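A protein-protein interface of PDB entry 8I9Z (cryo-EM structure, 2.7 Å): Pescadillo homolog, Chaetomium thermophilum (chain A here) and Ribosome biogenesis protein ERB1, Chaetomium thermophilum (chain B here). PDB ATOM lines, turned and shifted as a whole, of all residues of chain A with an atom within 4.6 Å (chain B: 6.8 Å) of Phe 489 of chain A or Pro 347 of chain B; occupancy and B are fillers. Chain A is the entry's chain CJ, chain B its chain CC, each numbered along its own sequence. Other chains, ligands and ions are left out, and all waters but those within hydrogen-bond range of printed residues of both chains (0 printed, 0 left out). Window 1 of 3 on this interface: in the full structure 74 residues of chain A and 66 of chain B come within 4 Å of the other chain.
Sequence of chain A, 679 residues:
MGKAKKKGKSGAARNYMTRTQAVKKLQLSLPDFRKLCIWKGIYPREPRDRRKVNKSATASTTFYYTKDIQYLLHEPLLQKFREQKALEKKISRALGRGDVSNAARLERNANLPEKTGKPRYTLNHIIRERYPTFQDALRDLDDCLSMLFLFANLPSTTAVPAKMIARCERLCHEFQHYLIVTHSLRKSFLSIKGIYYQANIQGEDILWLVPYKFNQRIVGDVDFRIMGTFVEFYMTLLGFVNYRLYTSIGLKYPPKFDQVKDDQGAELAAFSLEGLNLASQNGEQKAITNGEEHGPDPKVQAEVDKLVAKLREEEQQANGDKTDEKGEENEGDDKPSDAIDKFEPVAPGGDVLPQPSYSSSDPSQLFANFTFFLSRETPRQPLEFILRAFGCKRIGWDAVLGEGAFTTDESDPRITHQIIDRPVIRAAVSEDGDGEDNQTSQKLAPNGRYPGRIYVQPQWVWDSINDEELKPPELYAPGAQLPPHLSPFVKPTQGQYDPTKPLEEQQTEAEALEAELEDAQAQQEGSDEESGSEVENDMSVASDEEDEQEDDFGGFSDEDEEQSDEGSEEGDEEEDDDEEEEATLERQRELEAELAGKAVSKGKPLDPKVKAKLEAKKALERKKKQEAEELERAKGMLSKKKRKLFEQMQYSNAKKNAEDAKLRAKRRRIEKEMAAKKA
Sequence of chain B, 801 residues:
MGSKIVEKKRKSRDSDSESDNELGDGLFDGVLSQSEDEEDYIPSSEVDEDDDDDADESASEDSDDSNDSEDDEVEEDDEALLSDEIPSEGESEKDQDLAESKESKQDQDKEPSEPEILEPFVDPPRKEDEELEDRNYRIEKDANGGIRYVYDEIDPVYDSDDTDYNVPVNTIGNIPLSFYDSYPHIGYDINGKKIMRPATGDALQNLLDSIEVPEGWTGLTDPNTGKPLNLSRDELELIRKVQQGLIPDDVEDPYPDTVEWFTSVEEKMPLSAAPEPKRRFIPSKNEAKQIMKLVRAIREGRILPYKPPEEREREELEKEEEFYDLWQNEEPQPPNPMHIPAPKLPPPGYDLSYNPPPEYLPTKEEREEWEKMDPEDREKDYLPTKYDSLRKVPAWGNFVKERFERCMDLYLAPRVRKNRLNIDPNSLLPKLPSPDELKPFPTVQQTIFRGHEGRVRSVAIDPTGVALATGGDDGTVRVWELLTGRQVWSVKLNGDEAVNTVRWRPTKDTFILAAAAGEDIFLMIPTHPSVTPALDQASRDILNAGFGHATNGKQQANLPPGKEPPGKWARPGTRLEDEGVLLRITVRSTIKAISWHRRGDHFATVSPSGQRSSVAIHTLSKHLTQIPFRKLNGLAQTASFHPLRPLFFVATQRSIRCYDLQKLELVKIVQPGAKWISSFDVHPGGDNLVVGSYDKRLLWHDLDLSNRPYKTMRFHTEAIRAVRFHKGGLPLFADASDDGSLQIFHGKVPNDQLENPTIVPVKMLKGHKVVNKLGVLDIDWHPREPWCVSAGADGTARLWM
N of Tyr 196 of chain A is in hydrogen-bond range of O of Phe 189 of chain A (3.1 Å).
Phe 489 of chain A touches just these residues of chain B: Pro 347 and Pro 348.
Of chain A, only Phe 489 (3.6 Å) comes within 4 Å of Pro 347 of chain B.
Of the printed residues of chain B, Tyr 196 of chain A touches Pro 348.
Of the printed residues of chain B, Phe 189 of chain A touches Pro 348 and Gly 349.
Printed residues of chain A within 4 Å of Gly 349 of chain B: Phe 189, Ser 487 and Val 490.
Of the printed residues of chain A, Pro 348 of chain B touches Phe 189 (3.9 Å), Tyr 196 (3.6 Å), Ser 487 (3.8 Å), Phe 489 (3.5 Å) and Val 490 (3.5 Å).
Of the printed residues of chain B, Ser 487 of chain A touches Pro 348 and Gly 349.
Lys 344 of chain B touches none of the printed residues of chain A.
The nearest residue of chain A that does not touch Pro 347 of chain B is Leu 207 of chain A (4.5 Å).
Among the printed residues, merely in contact across the chains: Val 490 of chain A with Pro 348 of chain B, Phe 489 of chain A with Pro 348 of chain B, Phe 189 of chain A with Gly 349 of chain B, Phe 489 of chain A with Pro 347 of chain B, Tyr 196 of chain A with Pro 348 of chain B, Ser 487 of chain A with Gly 349 of chain B, Val 490 of chain A with Gly 349 of chain B, Ser 487 of chain A with Pro 348 of chain B and Phe 189 of chain A with Pro 348 of chain B.
Printed residues of chain B that touch a printed residue of chain A: Pro 347, Pro 348 and Gly 349.
Hydrophobic or aromatic side chains of chain B within 4 Å of the printed part of chain A: Pro 347 and Pro 348.
Among the printed residues, 9 pairs touch across the chains.
Among the printed residues, no Asp or Glu carboxylate lies within 4 Å of a Lys or Arg side-chain nitrogen of the other chain.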
ATOM      1  N   LYS A 187     -27.370  -2.438   6.280  1.00  0.00           N
ATOM      2  CA  LYS A 187     -26.280  -3.279   6.747  1.00  0.00           C
ATOM      3  C   LYS A 187     -26.194  -3.195   8.263  1.00  0.00           C
ATOM      4  O   LYS A 187     -26.709  -2.259   8.877  1.00  0.00           O
ATOM      5  CB  LYS A 187     -24.941  -2.854   6.133  1.00  0.00           C
ATOM      6  CG  LYS A 187     -24.449  -3.669   4.941  1.00  0.00           C
ATOM      7  CD  LYS A 187     -25.500  -3.963   3.899  1.00  0.00           C
ATOM      8  CE  LYS A 187     -24.872  -4.470   2.613  1.00  0.00           C
ATOM      9  NZ  LYS A 187     -23.911  -5.580   2.869  1.00  0.00           N
ATOM     10  N   PHE A 189     -23.456  -4.782  11.750  1.00  0.00           N
ATOM     11  CA  PHE A 189     -22.144  -5.320  12.068  1.00  0.00           C
ATOM     12  C   PHE A 189     -21.990  -5.463  13.574  1.00  0.00           C
ATOM     13  O   PHE A 189     -22.472  -4.632  14.345  1.00  0.00           O
ATOM     14  CB  PHE A 189     -21.052  -4.411  11.504  1.00  0.00           C
ATOM     15  CG  PHE A 189     -19.661  -4.929  11.685  1.00  0.00           C
ATOM     16  CD1 PHE A 189     -19.353  -6.256  11.469  1.00  0.00           C
ATOM     17  CD2 PHE A 189     -18.649  -4.067  12.061  1.00  0.00           C
ATOM     18  CE1 PHE A 189     -18.069  -6.710  11.640  1.00  0.00           C
ATOM     19  CE2 PHE A 189     -17.365  -4.518  12.228  1.00  0.00           C
ATOM     20  CZ  PHE A 189     -17.075  -5.837  12.017  1.00  0.00           C
ATOM     21  N   TYR A 196     -22.917  -1.646  14.862  1.00  0.00           N
ATOM     22  CA  TYR A 196     -22.975  -0.594  13.861  1.00  0.00           C
ATOM     23  C   TYR A 196     -24.180  -0.814  12.960  1.00  0.00           C
ATOM     24  O   TYR A 196     -24.428  -1.937  12.516  1.00  0.00           O
ATOM     25  CB  TYR A 196     -21.703  -0.570  13.019  1.00  0.00           C
ATOM     26  CG  TYR A 196     -20.481  -0.050  13.727  1.00  0.00           C
ATOM     27  CD1 TYR A 196     -20.182   1.303  13.731  1.00  0.00           C
ATOM     28  CD2 TYR A 196     -19.613  -0.912  14.367  1.00  0.00           C
ATOM     29  CE1 TYR A 196     -19.057   1.779  14.361  1.00  0.00           C
ATOM     30  CE2 TYR A 196     -18.488  -0.444  15.002  1.00  0.00           C
ATOM     31  CZ  TYR A 196     -18.213   0.898  14.994  1.00  0.00           C
ATOM     32  OH  TYR A 196     -17.090   1.367  15.633  1.00  0.00           O
ATOM     33  N   GLN A 198     -26.041   0.669   9.439  1.00  0.00           N
ATOM     34  CA  GLN A 198     -25.933   1.490   8.242  1.00  0.00           C
ATOM     35  C   GLN A 198     -27.295   1.553   7.576  1.00  0.00           C
ATOM     36  O   GLN A 198     -27.847   0.519   7.188  1.00  0.00           O
ATOM     37  CB  GLN A 198     -24.888   0.938   7.276  1.00  0.00           C
ATOM     38  CG  GLN A 198     -24.162   2.014   6.492  1.00  0.00           C
ATOM     39  CD  GLN A 198     -24.455   1.958   5.012  1.00  0.00           C
ATOM     40  OE1 GLN A 198     -25.570   1.644   4.598  1.00  0.00           O
ATOM     41  NE2 GLN A 198     -23.451   2.259   4.201  1.00  0.00           N
ATOM     42  N   LEU A 207     -24.310   5.928   9.356  1.00  0.00           N
ATOM     43  CA  LEU A 207     -23.677   4.888  10.152  1.00  0.00           C
ATOM     44  C   LEU A 207     -23.522   5.361  11.589  1.00  0.00           C
ATOM     45  O   LEU A 207     -22.814   6.337  11.851  1.00  0.00           O
ATOM     46  CB  LEU A 207     -22.318   4.509   9.570  1.00  0.00           C
ATOM     47  CG  LEU A 207     -21.523   3.486  10.370  1.00  0.00           C
ATOM     48  CD1 LEU A 207     -22.237   2.151  10.363  1.00  0.00           C
ATOM     49  CD2 LEU A 207     -20.123   3.351   9.808  1.00  0.00           C
ATOM     50  N   SER A 487     -17.028  -7.768   8.002  1.00  0.00           N
ATOM     51  CA  SER A 487     -17.459  -6.382   8.050  1.00  0.00           C
ATOM     52  C   SER A 487     -17.954  -5.956   6.682  1.00  0.00           C
ATOM     53  O   SER A 487     -17.196  -6.050   5.705  1.00  0.00           O
ATOM     54  CB  SER A 487     -16.315  -5.481   8.495  1.00  0.00           C
ATOM     55  OG  SER A 487     -15.524  -5.088   7.388  1.00  0.00           O
ATOM     56  N   PRO A 488     -19.195  -5.489   6.556  1.00  0.00           N
ATOM     57  CA  PRO A 488     -19.700  -5.112   5.231  1.00  0.00           C
ATOM     58  C   PRO A 488     -19.185  -3.776   4.737  1.00  0.00           C
ATOM     59  O   PRO A 488     -19.242  -3.520   3.529  1.00  0.00           O
ATOM     60  CB  PRO A 488     -21.216  -5.062   5.436  1.00  0.00           C
ATOM     61  CG  PRO A 488     -21.466  -5.598   6.815  1.00  0.00           C
ATOM     62  CD  PRO A 488     -20.228  -5.352   7.586  1.00  0.00           C
ATOM     63  N   PHE A 489     -18.688  -2.920   5.627  1.00  0.00           N
ATOM     64  CA  PHE A 489     -18.433  -1.533   5.264  1.00  0.00           C
ATOM     65  C   PHE A 489     -17.182  -1.355   4.419  1.00  0.00           C
ATOM     66  O   PHE A 489     -17.153  -0.476   3.550  1.00  0.00           O
ATOM     67  CB  PHE A 489     -18.340  -0.683   6.524  1.00  0.00           C
ATOM     68  CG  PHE A 489     -19.478  -0.887   7.466  1.00  0.00           C
ATOM     69  CD1 PHE A 489     -20.772  -0.624   7.065  1.00  0.00           C
ATOM     70  CD2 PHE A 489     -19.258  -1.354   8.743  1.00  0.00           C
ATOM     71  CE1 PHE A 489     -21.824  -0.812   7.925  1.00  0.00           C
ATOM     72  CE2 PHE A 489     -20.306  -1.537   9.608  1.00  0.00           C
ATOM     73  CZ  PHE A 489     -21.590  -1.271   9.199  1.00  0.00           C
ATOM     74  N   VAL A 490     -16.144  -2.155   4.651  1.00  0.00           N
ATOM     75  CA  VAL A 490     -14.918  -2.010   3.880  1.00  0.00           C
ATOM     76  C   VAL A 490     -15.144  -2.522   2.463  1.00  0.00           C
ATOM     77  O   VAL A 490     -16.011  -3.371   2.218  1.00  0.00           O
ATOM     78  CB  VAL A 490     -13.749  -2.725   4.576  1.00  0.00           C
ATOM     79  CG1 VAL A 490     -13.782  -2.443   6.065  1.00  0.00           C
ATOM     80  CG2 VAL A 490     -13.794  -4.207   4.330  1.00  0.00           C
ATOM     81  N   LYS A 491     -14.414  -1.955   1.516  1.00  0.00           N
ATOM     82  CA  LYS A 491     -14.531  -2.337   0.119  1.00  0.00           C
ATOM     83  C   LYS A 491     -13.264  -3.038  -0.351  1.00  0.00           C
ATOM     84  O   LYS A 491     -12.167  -2.711   0.116  1.00  0.00           O
ATOM     85  CB  LYS A 491     -14.794  -1.109  -0.755  1.00  0.00           C
ATOM     86  CG  LYS A 491     -13.943   0.101  -0.401  1.00  0.00           C
ATOM     87  CD  LYS A 491     -14.501   1.368  -1.032  1.00  0.00           C
ATOM     88  CE  LYS A 491     -15.925   1.637  -0.568  1.00  0.00           C
ATOM     89  NZ  LYS A 491     -16.009   1.786   0.912  1.00  0.00           N
ATOM     90  N   LYS B 344     -15.113  12.542   8.440  1.00  0.00           N
ATOM     91  CA  LYS B 344     -15.838  11.406   8.983  1.00  0.00           C
ATOM     92  C   LYS B 344     -14.869  10.367   9.528  1.00  0.00           C
ATOM     93  O   LYS B 344     -13.751  10.208   9.029  1.00  0.00           O
ATOM     94  CB  LYS B 344     -16.728  10.778   7.911  1.00  0.00           C
ATOM     95  CG  LYS B 344     -18.027  11.521   7.671  1.00  0.00           C
ATOM     96  CD  LYS B 344     -19.193  10.568   7.480  1.00  0.00           C
ATOM     97  CE  LYS B 344     -19.134   9.897   6.117  1.00  0.00           C
ATOM     98  NZ  LYS B 344     -20.326   9.042   5.872  1.00  0.00           N
ATOM     99  N   LEU B 345     -15.308   9.663  10.569  1.00  0.00           N
ATOM    100  CA  LEU B 345     -14.540   8.545  11.093  1.00  0.00           C
ATOM    101  C   LEU B 345     -14.487   7.429  10.052  1.00  0.00           C
ATOM    102  O   LEU B 345     -15.402   7.291   9.239  1.00  0.00           O
ATOM    103  CB  LEU B 345     -15.151   7.998  12.387  1.00  0.00           C
ATOM    104  CG  LEU B 345     -15.137   8.672  13.771  1.00  0.00           C
ATOM    105  CD1 LEU B 345     -15.367  10.168  13.754  1.00  0.00           C
ATOM    106  CD2 LEU B 345     -16.132   7.994  14.711  1.00  0.00           C
ATOM    107  N   PRO B 346     -13.408   6.640  10.033  1.00  0.00           N
ATOM    108  CA  PRO B 346     -13.356   5.515   9.108  1.00  0.00           C
ATOM    109  C   PRO B 346     -14.385   4.466   9.478  1.00  0.00           C
ATOM    110  O   PRO B 346     -14.716   4.290  10.664  1.00  0.00           O
ATOM    111  CB  PRO B 346     -11.923   4.978   9.283  1.00  0.00           C
ATOM    112  CG  PRO B 346     -11.165   6.085   9.920  1.00  0.00           C
ATOM    113  CD  PRO B 346     -12.149   6.796  10.780  1.00  0.00           C
ATOM    114  N   PRO B 347     -14.945   3.759   8.493  1.00  0.00           N
ATOM    115  CA  PRO B 347     -15.841   2.653   8.811  1.00  0.00           C
ATOM    116  C   PRO B 347     -15.078   1.525   9.478  1.00  0.00           C
ATOM    117  O   PRO B 347     -13.876   1.335   9.226  1.00  0.00           O
ATOM    118  CB  PRO B 347     -16.381   2.230   7.434  1.00  0.00           C
ATOM    119  CG  PRO B 347     -15.369   2.713   6.467  1.00  0.00           C
ATOM    120  CD  PRO B 347     -14.820   3.976   7.044  1.00  0.00           C
ATOM    121  N   PRO B 348     -15.725   0.763  10.360  1.00  0.00           N
ATOM    122  CA  PRO B 348     -15.016  -0.301  11.077  1.00  0.00           C
ATOM    123  C   PRO B 348     -14.597  -1.429  10.147  1.00  0.00           C
ATOM    124  O   PRO B 348     -15.284  -1.755   9.178  1.00  0.00           O
ATOM    125  CB  PRO B 348     -16.039  -0.780  12.108  1.00  0.00           C
ATOM    126  CG  PRO B 348     -17.348  -0.392  11.551  1.00  0.00           C
ATOM    127  CD  PRO B 348     -17.134   0.864  10.773  1.00  0.00           C
ATOM    128  N   GLY B 349     -13.442  -2.020  10.450  1.00  0.00           N
ATOM    129  CA  GLY B 349     -12.861  -3.048   9.620  1.00  0.00           C
ATOM    130  C   GLY B 349     -13.105  -4.450  10.155  1.00  0.00           C
ATOM    131  O   GLY B 349     -13.848  -4.673  11.107  1.00  0.00           O
ATOM    132  N   LEU B 352     -12.236  -5.260  14.009  1.00  0.00           N
ATOM    133  CA  LEU B 352     -13.077  -4.913  15.141  1.00  0.00           C
ATOM    134  C   LEU B 352     -14.115  -5.971  15.472  1.00  0.00           C
ATOM    135  O   LEU B 352     -14.669  -5.935  16.574  1.00  0.00           O
ATOM    136  CB  LEU B 352     -13.772  -3.578  14.881  1.00  0.00           C
ATOM    137  CG  LEU B 352     -13.017  -2.358  15.402  1.00  0.00           C
ATOM    138  CD1 LEU B 352     -13.694  -1.078  14.962  1.00  0.00           C
ATOM    139  CD2 LEU B 352     -12.912  -2.415  16.913  1.00  0.00           C
